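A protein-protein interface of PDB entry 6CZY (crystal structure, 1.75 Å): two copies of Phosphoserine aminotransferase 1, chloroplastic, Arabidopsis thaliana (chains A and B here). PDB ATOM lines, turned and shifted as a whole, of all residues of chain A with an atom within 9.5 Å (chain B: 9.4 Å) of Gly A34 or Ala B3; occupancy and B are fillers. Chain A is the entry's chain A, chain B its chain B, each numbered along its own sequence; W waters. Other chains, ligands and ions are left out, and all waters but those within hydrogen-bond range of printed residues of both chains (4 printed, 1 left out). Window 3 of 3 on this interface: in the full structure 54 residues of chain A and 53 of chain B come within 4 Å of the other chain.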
ATOM      1  N   ASP A  26       2.936 -26.538  19.522  1.00  0.00           N
ATOM      2  CA  ASP A  26       2.227 -27.110  18.368  1.00  0.00           C
ATOM      3  C   ASP A  26       0.797 -26.569  18.250  1.00  0.00           C
ATOM      4  O   ASP A  26       0.086 -26.962  17.377  1.00  0.00           O
ATOM      5  CB  ASP A  26       2.220 -28.660  18.431  1.00  0.00           C
ATOM      6  CG  ASP A  26       3.606 -29.277  18.160  1.00  0.00           C
ATOM      7  OD1 ASP A  26       4.541 -28.513  17.771  1.00  0.00           O
ATOM      8  OD2 ASP A  26       3.817 -30.478  18.399  1.00  0.00           O
ATOM      9  N   LEU A  27       0.384 -25.651  19.124  1.00  0.00           N
ATOM     10  CA  LEU A  27      -1.031 -25.304  19.238  1.00  0.00           C
ATOM     11  C   LEU A  27      -1.653 -24.631  18.009  1.00  0.00           C
ATOM     12  O   LEU A  27      -2.857 -24.783  17.726  1.00  0.00           O
ATOM     13  CB  LEU A  27      -1.263 -24.395  20.458  1.00  0.00           C
ATOM     14  CG  LEU A  27      -2.694 -24.416  21.054  1.00  0.00           C
ATOM     15  CD1 LEU A  27      -2.944 -25.748  21.696  1.00  0.00           C
ATOM     16  CD2 LEU A  27      -2.903 -23.291  22.090  1.00  0.00           C
ATOM     17  N   TYR A  28      -0.851 -23.854  17.294  1.00  0.00           N
ATOM     18  CA  TYR A  28      -1.326 -23.087  16.147  1.00  0.00           C
ATOM     19  C   TYR A  28      -1.354 -23.880  14.858  1.00  0.00           C
ATOM     20  O   TYR A  28      -2.150 -23.623  13.955  1.00  0.00           O
ATOM     21  CB  TYR A  28      -0.395 -21.879  15.985  1.00  0.00           C
ATOM     22  CG  TYR A  28      -0.883 -20.809  15.068  1.00  0.00           C
ATOM     23  CD1 TYR A  28      -2.063 -20.099  15.342  1.00  0.00           C
ATOM     24  CD2 TYR A  28      -0.141 -20.436  13.953  1.00  0.00           C
ATOM     25  CE1 TYR A  28      -2.473 -19.068  14.525  1.00  0.00           C
ATOM     26  CE2 TYR A  28      -0.571 -19.406  13.120  1.00  0.00           C
ATOM     27  CZ  TYR A  28      -1.732 -18.734  13.422  1.00  0.00           C
ATOM     28  OH  TYR A  28      -2.163 -17.720  12.609  1.00  0.00           O
ATOM     29  N   ASN A  29      -0.428 -24.817  14.756  1.00  0.00           N
ATOM     30  CA  ASN A  29      -0.233 -25.610  13.540  1.00  0.00           C
ATOM     31  C   ASN A  29       0.475 -26.906  13.914  1.00  0.00           C
ATOM     32  O   ASN A  29       1.697 -26.910  14.080  1.00  0.00           O
ATOM     33  CB  ASN A  29       0.603 -24.795  12.538  1.00  0.00           C
ATOM     34  CG  ASN A  29       0.750 -25.498  11.199  1.00  0.00           C
ATOM     35  OD1 ASN A  29       0.571 -26.732  11.105  1.00  0.00           O
ATOM     36  ND2 ASN A  29       1.095 -24.718  10.133  1.00  0.00           N
ATOM     37  N   TRP A  30      -0.269 -28.003  14.058  1.00  0.00           N
ATOM     38  CA  TRP A  30       0.314 -29.259  14.521  1.00  0.00           C
ATOM     39  C   TRP A  30       1.066 -29.953  13.365  1.00  0.00           C
ATOM     40  O   TRP A  30       0.462 -30.402  12.426  1.00  0.00           O
ATOM     41  CB  TRP A  30      -0.770 -30.190  15.040  1.00  0.00           C
ATOM     42  CG  TRP A  30      -0.334 -31.514  15.619  1.00  0.00           C
ATOM     43  CD1 TRP A  30       0.094 -31.745  16.888  1.00  0.00           C
ATOM     44  CD2 TRP A  30      -0.361 -32.793  14.971  1.00  0.00           C
ATOM     45  NE1 TRP A  30       0.364 -33.091  17.058  1.00  0.00           N
ATOM     46  CE2 TRP A  30       0.081 -33.751  15.903  1.00  0.00           C
ATOM     47  CE3 TRP A  30      -0.709 -33.221  13.691  1.00  0.00           C
ATOM     48  CZ2 TRP A  30       0.202 -35.112  15.589  1.00  0.00           C
ATOM     49  CZ3 TRP A  30      -0.609 -34.551  13.383  1.00  0.00           C
ATOM     50  CH2 TRP A  30      -0.155 -35.487  14.328  1.00  0.00           C
ATOM     51  N   ARG A  31       2.381 -30.051  13.490  1.00  0.00           N
ATOM     52  CA  ARG A  31       3.211 -30.820  12.555  1.00  0.00           C
ATOM     53  C   ARG A  31       2.991 -30.518  11.055  1.00  0.00           C
ATOM     54  O   ARG A  31       2.797 -31.446  10.263  1.00  0.00           O
ATOM     55  CB  ARG A  31       2.931 -32.296  12.797  1.00  0.00           C
ATOM     56  CG  ARG A  31       3.445 -32.769  14.129  1.00  0.00           C
ATOM     57  CD  ARG A  31       3.498 -34.271  14.219  1.00  0.00           C
ATOM     58  NE  ARG A  31       3.792 -34.658  15.595  1.00  0.00           N
ATOM     59  CZ  ARG A  31       3.724 -35.907  16.082  1.00  0.00           C
ATOM     60  NH1 ARG A  31       3.999 -36.162  17.349  1.00  0.00           N
ATOM     61  NH2 ARG A  31       3.367 -36.906  15.285  1.00  0.00           N
ATOM     62  N   GLY A  32       2.927 -29.253  10.696  1.00  0.00           N
ATOM     63  CA  GLY A  32       2.633 -28.834   9.301  1.00  0.00           C
ATOM     64  C   GLY A  32       1.321 -29.339   8.691  1.00  0.00           C
ATOM     65  O   GLY A  32       1.131 -29.270   7.455  1.00  0.00           O
ATOM     66  N   SER A  33       0.412 -29.836   9.520  1.00  0.00           N
ATOM     67  CA  SER A  33      -0.909 -30.193   9.041  1.00  0.00           C
ATOM     68  C   SER A  33      -1.687 -28.968   8.614  1.00  0.00           C
ATOM     69  O   SER A  33      -2.701 -29.090   7.941  1.00  0.00           O
ATOM     70  CB  SER A  33      -1.704 -30.901  10.126  1.00  0.00           C
ATOM     71  OG  SER A  33      -2.005 -30.008  11.179  1.00  0.00           O
ATOM     72  N   GLY A  34      -1.277 -27.793   9.079  1.00  0.00           N
ATOM     73  CA  GLY A  34      -1.956 -26.561   8.733  1.00  0.00           C
ATOM     74  C   GLY A  34      -3.104 -26.130   9.632  1.00  0.00           C
ATOM     75  O   GLY A  34      -3.845 -25.213   9.273  1.00  0.00           O
ATOM     76  N   MET A  35      -3.224 -26.778  10.795  1.00  0.00           N
ATOM     77  CA  MET A  35      -4.250 -26.418  11.754  1.00  0.00           C
ATOM     78  C   MET A  35      -3.887 -26.906  13.138  1.00  0.00           C
ATOM     79  O   MET A  35      -2.954 -27.730  13.321  1.00  0.00           O
ATOM     80  CB  MET A  35      -5.584 -27.028  11.321  1.00  0.00           C
ATOM     81  CG  MET A  35      -5.568 -28.547  11.311  1.00  0.00           C
ATOM     82  SD  MET A  35      -7.080 -29.291  10.616  1.00  0.00           S
ATOM     83  CE  MET A  35      -6.763 -29.083   8.851  1.00  0.00           C
ATOM     84  N   SER A  36      -4.619 -26.394  14.134  1.00  0.00           N
ATOM     85  CA  SER A  36      -4.501 -26.848  15.507  1.00  0.00           C
ATOM     86  C   SER A  36      -5.180 -28.197  15.668  1.00  0.00           C
ATOM     87  O   SER A  36      -6.176 -28.451  14.989  1.00  0.00           O
ATOM     88  CB  SER A  36      -5.218 -25.832  16.442  1.00  0.00           C
ATOM     89  OG  SER A  36      -5.123 -26.186  17.809  1.00  0.00           O
ATOM     90  N   VAL A  37      -4.725 -28.976  16.643  1.00  0.00           N
ATOM     91  CA  VAL A  37      -5.477 -30.160  17.111  1.00  0.00           C
ATOM     92  C   VAL A  37      -6.923 -29.764  17.427  1.00  0.00           C
ATOM     93  O   VAL A  37      -7.838 -30.547  17.132  1.00  0.00           O
ATOM     94  CB  VAL A  37      -4.815 -30.850  18.305  1.00  0.00           C
ATOM     95  CG1 VAL A  37      -5.761 -31.910  18.901  1.00  0.00           C
ATOM     96  CG2 VAL A  37      -3.503 -31.492  17.879  1.00  0.00           C
ATOM     97  N   GLU A  39      -8.875 -27.870  15.905  1.00  0.00           N
ATOM     98  CA  GLU A  39      -9.605 -27.619  14.674  1.00  0.00           C
ATOM     99  C   GLU A  39      -9.730 -28.841  13.760  1.00  0.00           C
ATOM    100  O   GLU A  39     -10.330 -28.707  12.684  1.00  0.00           O
ATOM    101  CB  GLU A  39      -8.919 -26.508  13.863  1.00  0.00           C
ATOM    102  CG  GLU A  39      -8.854 -25.159  14.560  1.00  0.00           C
ATOM    103  CD  GLU A  39      -7.875 -24.208  13.890  1.00  0.00           C
ATOM    104  OE1 GLU A  39      -6.672 -24.544  13.844  1.00  0.00           O
ATOM    105  OE2 GLU A  39      -8.301 -23.137  13.389  1.00  0.00           O
ATOM    106  N   MET A  40      -9.159 -29.978  14.174  1.00  0.00           N
ATOM    107  CA  MET A  40      -9.053 -31.156  13.310  1.00  0.00           C
ATOM    108  C   MET A  40     -10.373 -31.923  13.251  1.00  0.00           C
ATOM    109  O   MET A  40     -11.014 -32.111  14.270  1.00  0.00           O
ATOM    110  CB  MET A  40      -8.022 -32.137  13.862  1.00  0.00           C
ATOM    111  CG  MET A  40      -6.596 -31.707  13.669  1.00  0.00           C
ATOM    112  SD  MET A  40      -5.511 -32.880  14.453  1.00  0.00           S
ATOM    113  CE  MET A  40      -4.003 -32.018  14.110  1.00  0.00           C
ATOM    114  N   LYS A  45      -7.241 -38.007   9.000  1.00  0.00           N
ATOM    115  CA  LYS A  45      -6.073 -38.842   9.248  1.00  0.00           C
ATOM    116  C   LYS A  45      -5.180 -38.334  10.370  1.00  0.00           C
ATOM    117  O   LYS A  45      -4.609 -39.147  11.074  1.00  0.00           O
ATOM    118  CB  LYS A  45      -5.259 -39.073   7.956  1.00  0.00           C
ATOM    119  CG  LYS A  45      -4.434 -37.895   7.512  1.00  0.00           C
ATOM    120  CD  LYS A  45      -3.652 -38.238   6.233  1.00  0.00           C
ATOM    121  CE  LYS A  45      -2.849 -37.042   5.737  1.00  0.00           C
ATOM    122  NZ  LYS A  45      -3.773 -35.925   5.364  1.00  0.00           N
ATOM    123  N   GLU A  46      -5.065 -37.013  10.571  1.00  0.00           N
ATOM    124  CA  GLU A  46      -4.215 -36.532  11.651  1.00  0.00           C
ATOM    125  C   GLU A  46      -4.802 -36.957  12.995  1.00  0.00           C
ATOM    126  O   GLU A  46      -4.106 -37.495  13.845  1.00  0.00           O
ATOM    127  CB  GLU A  46      -3.988 -35.028  11.630  1.00  0.00           C
ATOM    128  CG  GLU A  46      -3.155 -34.589  10.441  1.00  0.00           C
ATOM    129  CD  GLU A  46      -3.949 -34.423   9.185  1.00  0.00           C
ATOM    130  OE1 GLU A  46      -5.175 -34.675   9.147  1.00  0.00           O
ATOM    131  OE2 GLU A  46      -3.300 -34.002   8.219  1.00  0.00           O
ATOM    132  N   ASN B   2       4.584 -25.910   6.984  1.00  0.00           N
ATOM    133  CA  ASN B   2       3.997 -24.962   5.984  1.00  0.00           C
ATOM    134  C   ASN B   2       2.842 -24.177   6.670  1.00  0.00           C
ATOM    135  O   ASN B   2       2.485 -24.473   7.794  1.00  0.00           O
ATOM    136  CB  ASN B   2       3.547 -25.732   4.718  1.00  0.00           C
ATOM    137  CG  ASN B   2       3.796 -24.960   3.418  1.00  0.00           C
ATOM    138  OD1 ASN B   2       3.129 -23.953   3.124  1.00  0.00           O
ATOM    139  ND2 ASN B   2       4.729 -25.459   2.609  1.00  0.00           N
ATOM    140  N   ALA B   3       2.301 -23.177   5.989  1.00  0.00           N
ATOM    141  CA  ALA B   3       1.305 -22.261   6.511  1.00  0.00           C
ATOM    142  C   ALA B   3      -0.046 -22.924   6.880  1.00  0.00           C
ATOM    143  O   ALA B   3      -0.332 -24.050   6.455  1.00  0.00           O
ATOM    144  CB  ALA B   3       1.042 -21.152   5.505  1.00  0.00           C
ATOM    145  N   ARG B   4      -0.881 -22.148   7.564  1.00  0.00           N
ATOM    146  CA  ARG B   4      -2.225 -22.618   7.895  1.00  0.00           C
ATOM    147  C   ARG B   4      -3.077 -22.749   6.649  1.00  0.00           C
ATOM    148  O   ARG B   4      -2.987 -21.933   5.740  1.00  0.00           O
ATOM    149  CB  ARG B   4      -2.870 -21.710   8.927  1.00  0.00           C
ATOM    150  CG  ARG B   4      -2.399 -22.186  10.319  1.00  0.00           C
ATOM    151  CD  ARG B   4      -2.809 -21.228  11.413  1.00  0.00           C
ATOM    152  NE  ARG B   4      -4.253 -21.076  11.418  1.00  0.00           N
ATOM    153  CZ  ARG B   4      -5.090 -21.862  12.088  1.00  0.00           C
ATOM    154  NH1 ARG B   4      -4.657 -22.839  12.842  1.00  0.00           N
ATOM    155  NH2 ARG B   4      -6.410 -21.631  11.996  1.00  0.00           N
ATOM    156  N   VAL B   5      -3.876 -23.805   6.604  1.00  0.00           N
ATOM    157  CA  VAL B   5      -4.709 -24.067   5.425  1.00  0.00           C
ATOM    158  C   VAL B   5      -6.098 -23.444   5.583  1.00  0.00           C
ATOM    159  O   VAL B   5      -6.456 -22.982   6.657  1.00  0.00           O
ATOM    160  CB  VAL B   5      -4.857 -25.581   5.153  1.00  0.00           C
ATOM    161  CG1 VAL B   5      -3.505 -26.187   4.850  1.00  0.00           C
ATOM    162  CG2 VAL B   5      -5.484 -26.317   6.318  1.00  0.00           C
ATOM    163  N   PHE B   6      -6.873 -23.440   4.516  1.00  0.00           N
ATOM    164  CA  PHE B   6      -8.277 -23.076   4.615  1.00  0.00           C
ATOM    165  C   PHE B   6      -8.999 -24.351   4.959  1.00  0.00           C
ATOM    166  O   PHE B   6      -9.012 -25.272   4.190  1.00  0.00           O
ATOM    167  CB  PHE B   6      -8.784 -22.421   3.364  1.00  0.00           C
ATOM    168  CG  PHE B   6      -8.179 -21.034   3.123  1.00  0.00           C
ATOM    169  CD1 PHE B   6      -8.407 -20.019   4.032  1.00  0.00           C
ATOM    170  CD2 PHE B   6      -7.514 -20.748   1.956  1.00  0.00           C
ATOM    171  CE1 PHE B   6      -7.882 -18.742   3.829  1.00  0.00           C
ATOM    172  CE2 PHE B   6      -6.977 -19.484   1.735  1.00  0.00           C
ATOM    173  CZ  PHE B   6      -7.187 -18.469   2.657  1.00  0.00           C
ATOM    174  N   ASN B   7      -9.568 -24.405   6.162  1.00  0.00           N
ATOM    175  CA  ASN B   7     -10.109 -25.667   6.710  1.00  0.00           C
ATOM    176  C   ASN B   7     -11.637 -25.648   6.732  1.00  0.00           C
ATOM    177  O   ASN B   7     -12.262 -24.986   7.569  1.00  0.00           O
ATOM    178  CB  ASN B   7      -9.542 -25.855   8.120  1.00  0.00           C
ATOM    179  CG  ASN B   7     -10.124 -27.023   8.890  1.00  0.00           C
ATOM    180  OD1 ASN B   7     -10.758 -27.942   8.351  1.00  0.00           O
ATOM    181  ND2 ASN B   7      -9.907 -26.969  10.202  1.00  0.00           N
ATOM    182  N   PHE B   8     -12.210 -26.371   5.785  1.00  0.00           N
ATOM    183  CA  PHE B   8     -13.640 -26.462   5.600  1.00  0.00           C
ATOM    184  C   PHE B   8     -14.341 -27.555   6.399  1.00  0.00           C
ATOM    185  O   PHE B   8     -15.500 -27.861   6.096  1.00  0.00           O
ATOM    186  CB  PHE B   8     -14.008 -26.556   4.111  1.00  0.00           C
ATOM    187  CG  PHE B   8     -13.673 -25.314   3.331  1.00  0.00           C
ATOM    188  CD1 PHE B   8     -12.408 -25.130   2.809  1.00  0.00           C
ATOM    189  CD2 PHE B   8     -14.580 -24.318   3.169  1.00  0.00           C
ATOM    190  CE1 PHE B   8     -12.073 -23.973   2.111  1.00  0.00           C
ATOM    191  CE2 PHE B   8     -14.248 -23.143   2.494  1.00  0.00           C
ATOM    192  CZ  PHE B   8     -12.999 -22.982   1.944  1.00  0.00           C
ATOM    193  N   THR B  14     -12.557 -24.876  12.051  1.00  0.00           N
ATOM    194  CA  THR B  14     -11.625 -23.725  12.104  1.00  0.00           C
ATOM    195  C   THR B  14     -12.031 -22.729  13.224  1.00  0.00           C
ATOM    196  O   THR B  14     -13.216 -22.549  13.529  1.00  0.00           O
ATOM    197  CB  THR B  14     -11.549 -23.098  10.702  1.00  0.00           C
ATOM    198  OG1 THR B  14     -10.354 -22.303  10.572  1.00  0.00           O
ATOM    199  CG2 THR B  14     -12.747 -22.265  10.399  1.00  0.00           C
ATOM    200  N   LEU B  15     -11.024 -22.127  13.882  1.00  0.00           N
ATOM    201  CA  LEU B  15     -11.202 -21.212  15.017  1.00  0.00           C
ATOM    202  C   LEU B  15     -10.422 -19.929  14.739  1.00  0.00           C
ATOM    203  O   LEU B  15      -9.545 -19.966  13.916  1.00  0.00           O
ATOM    204  CB  LEU B  15     -10.661 -21.852  16.302  1.00  0.00           C
ATOM    205  CG  LEU B  15     -11.528 -22.967  16.890  1.00  0.00           C
ATOM    206  CD1 LEU B  15     -10.849 -23.648  18.042  1.00  0.00           C
ATOM    207  CD2 LEU B  15     -12.839 -22.395  17.372  1.00  0.00           C
ATOM    208  N   GLU B  17      -7.745 -17.179  14.505  1.00  0.00           N
ATOM    209  CA  GLU B  17      -6.298 -17.263  14.747  1.00  0.00           C
ATOM    210  C   GLU B  17      -5.883 -16.452  15.981  1.00  0.00           C
ATOM    211  O   GLU B  17      -5.029 -16.898  16.730  1.00  0.00           O
ATOM    212  CB  GLU B  17      -5.483 -16.837  13.510  1.00  0.00           C
ATOM    213  CG  GLU B  17      -5.600 -17.866  12.405  1.00  0.00           C
ATOM    214  CD  GLU B  17      -4.937 -17.522  11.084  1.00  0.00           C
ATOM    215  OE1 GLU B  17      -4.486 -16.376  10.909  1.00  0.00           O
ATOM    216  OE2 GLU B  17      -4.851 -18.431  10.233  1.00  0.00           O
ATOM    217  N   LEU B  20      -6.546 -18.623  18.970  1.00  0.00           N
ATOM    218  CA  LEU B  20      -5.585 -19.672  19.112  1.00  0.00           C
ATOM    219  C   LEU B  20      -4.257 -19.149  19.692  1.00  0.00           C
ATOM    220  O   LEU B  20      -3.638 -19.782  20.539  1.00  0.00           O
ATOM    221  CB  LEU B  20      -5.306 -20.368  17.769  1.00  0.00           C
ATOM    222  CG  LEU B  20      -6.466 -21.161  17.166  1.00  0.00           C
ATOM    223  CD1 LEU B  20      -6.142 -21.583  15.737  1.00  0.00           C
ATOM    224  CD2 LEU B  20      -6.851 -22.361  17.985  1.00  0.00           C
ATOM    225  N   LYS B 321      -4.628 -25.886  -0.772  1.00  0.00           N
ATOM    226  CA  LYS B 321      -4.784 -25.534   0.670  1.00  0.00           C
ATOM    227  C   LYS B 321      -6.222 -25.308   1.126  1.00  0.00           C
ATOM    228  O   LYS B 321      -6.472 -24.563   2.115  1.00  0.00           O
ATOM    229  CB  LYS B 321      -3.906 -24.332   1.030  1.00  0.00           C
ATOM    230  CG  LYS B 321      -2.463 -24.466   0.543  1.00  0.00           C
ATOM    231  CD  LYS B 321      -1.697 -25.466   1.384  1.00  0.00           C
ATOM    232  CE  LYS B 321      -1.867 -26.923   1.010  1.00  0.00           C
ATOM    233  NZ  LYS B 321      -0.549 -27.637   1.113  1.00  0.00           N
ATOM    234  N   MET B 322      -7.160 -25.993   0.443  1.00  0.00           N
ATOM    235  CA  MET B 322      -8.569 -25.941   0.804  1.00  0.00           C
ATOM    236  C   MET B 322      -8.994 -27.385   1.081  1.00  0.00           C
ATOM    237  O   MET B 322      -9.123 -28.184   0.153  1.00  0.00           O
ATOM    238  CB  MET B 322      -9.383 -25.283  -0.325  1.00  0.00           C
ATOM    239  CG  MET B 322      -9.064 -23.792  -0.554  1.00  0.00           C
ATOM    240  SD  MET B 322      -9.891 -23.103  -2.018  1.00  0.00           S
ATOM    241  CE  MET B 322      -8.964 -23.882  -3.321  1.00  0.00           C
ATOM    242  N   VAL B 323      -9.084 -27.737   2.363  1.00  0.00           N
ATOM    243  CA  VAL B 323      -9.211 -29.140   2.784  1.00  0.00           C
ATOM    244  C   VAL B 323     -10.587 -29.417   3.377  1.00  0.00           C
ATOM    245  O   VAL B 323     -11.240 -28.480   3.848  1.00  0.00           O
ATOM    246  CB  VAL B 323      -8.124 -29.517   3.795  1.00  0.00           C
ATOM    247  CG1 VAL B 323      -6.757 -29.216   3.181  1.00  0.00           C
ATOM    248  CG2 VAL B 323      -8.265 -28.739   5.096  1.00  0.00           C
ATOM    249  N   LYS B 349     -11.019 -17.761  -2.222  1.00  0.00           N
ATOM    250  CA  LYS B 349     -10.136 -18.719  -2.864  1.00  0.00           C
ATOM    251  C   LYS B 349     -10.915 -19.888  -3.452  1.00  0.00           C
ATOM    252  O   LYS B 349     -10.682 -20.287  -4.588  1.00  0.00           O
ATOM    253  CB  LYS B 349      -9.069 -19.231  -1.907  1.00  0.00           C
ATOM    254  CG  LYS B 349      -7.950 -19.916  -2.672  1.00  0.00           C
ATOM    255  CD  LYS B 349      -6.784 -20.368  -1.827  1.00  0.00           C
ATOM    256  CE  LYS B 349      -5.634 -20.732  -2.769  1.00  0.00           C
ATOM    257  NZ  LYS B 349      -4.524 -21.352  -1.995  1.00  0.00           N
HETATM  258  O   HOH W   1      -6.264 -24.019   9.310  1.00  0.00           O
HETATM  259  O   HOH W   2      -3.060 -14.554  12.604  1.00  0.00           O
HETATM  260  O   HOH W   3       3.179 -28.686   5.524  1.00  0.00           O
HETATM  261  O   HOH W   4      -8.452 -24.377  10.828  1.00  0.00           O
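O of Tyr A28 sits at hydrogen-bond distance from NH1 of Arg B4 (2.9 Å).
The side-chain hydroxyl (OH) of Tyr A28 lies close to the side-chain carboxylate (OE1) of Glu B17.
The side-chain amide nitrogen (ND2) of Asn A29 is in hydrogen-bond range of the backbone carbonyl oxygen (O) of Asn B2, 2.7 Å away.
O of Gly A34 is in hydrogen-bond range of N of Val B5 (3.0 Å).
ND2 of Asn B7 lies within hydrogen-bond range of SD of Met A35.
The side-chain carboxylate (OE2) of Glu A39 is in salt-bridge range of the guanidinium group (NH2) of Arg B4 (2.8 Å).
The backbone carbonyl oxygen (O) of Glu A39 is in hydrogen-bond range of the side-chain amide nitrogen (ND2) of Asn B7 (3.1 Å).
N of Leu B15 sits at hydrogen-bond distance from OE2 of Glu A39 (2.9 Å).
The side-chain hydroxyl (OG) of Ser A36 sits at hydrogen-bond distance from the backbone carbonyl oxygen (O) of Leu A27 (2.7 Å).
OD1 of Asn A29 is in hydrogen-bond range of N of Ser A33, 3.5 Å away.
The side-chain amide oxygen of Asn A29 is in hydrogen-bond range of the backbone NH of Gly A34 (2.9 Å).
The backbone carbonyl oxygen (O) of Met A35 is in hydrogen-bond range of the backbone NH (N) of Trp A30.
The side-chain hydroxyl (OG) of Ser A33 sits at hydrogen-bond distance from the backbone carbonyl oxygen (O) of Met A35, 3.3 Å away.
OE1 of Glu A39 is in hydrogen-bond range of N of Ser A36, at 2.8 Å.
Among the printed residues, pairs that only touch across the chains: Leu A27 with Leu B20 (3.9 Å), Asn A29 with Ala B3 (3.9 Å), Gly A34 with Ala B3 (3.8 Å), Gly A34 with Arg B4 (3.4 Å), Met A35 with Arg B4 (3.8 Å), Met A35 with Val B5 (3.96 Å), Ser A36 with Arg B4 (3.8 Å), Glu A39 with Thr B14 (3.6 Å) and Glu A39 with Leu B20 (3.5 Å).
Of the printed residues of chain B, Asn A29 touches Asn B2 (2.7 Å) and Ala B3 (3.9 Å).
Trp A30 touches none of the printed residues of chain B.
No residue of chain B comes within 4 Å of Gly A32.
No residue of chain B comes within 4 Å of Ser A33.
Met A35 touches three residues of chain B.
Of the printed residues of chain B, Glu A39 touches Arg B4 (2.8 Å), Asn B7 (3.1 Å), Thr B14 (3.6 Å), Leu B15 (2.9 Å) and Leu B20 (3.5 Å).
Of the printed residues of chain A, Asn B2 touches Asn A29 (2.7 Å).
Ala B3 touches two residues of chain A.
Arg B4 touches just these residues of chain A: Tyr A28 (2.9 Å), Gly A34 (3.4 Å), Met A35 (3.8 Å), Ser A36 (3.8 Å) and Glu A39 (2.8 Å).
Of chain A, only Gly A34 and Met A35 come within 4 Å of Val B5.
Printed residues of chain A within 4 Å of Thr B14: Glu A39 (3.6 Å).
Printed residues of chain A within 4 Å of Glu B17: Tyr A28 (3.2 Å).
The nearest printed residue of chain A that does not touch Ala B3 is Gly A32 (5.5 Å).
Hydrophobic or aromatic side chains of chain A within 4 Å of the printed part of chain B: Leu A27, Tyr A28 and Met A35.
Hydrophobic or aromatic side chains of chain B that line the printed part of chain A: Val B5, Leu B15 and Leu B20.
No position is printed for both chains.
Of the 17 pairs that touch across the chains among the printed residues, none has its exchanged pair printed and touching as well.
Water W1 bridges O of Gly A34 and O of Val B5.
Water W4 lies within hydrogen-bond range of OG1 of Thr B14, OE2 of Glu A39 and ND2 of Asn B7.
Water W2 lies within hydrogen-bond range of the side-chain carboxylate of Glu B17 (2.9 Å) and the side-chain hydroxyl of Tyr A28 (3.3 Å).
Water W3 bridges the backbone carbonyl oxygen (O) of Gly A32 and the backbone NH (N) of Asn B2.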
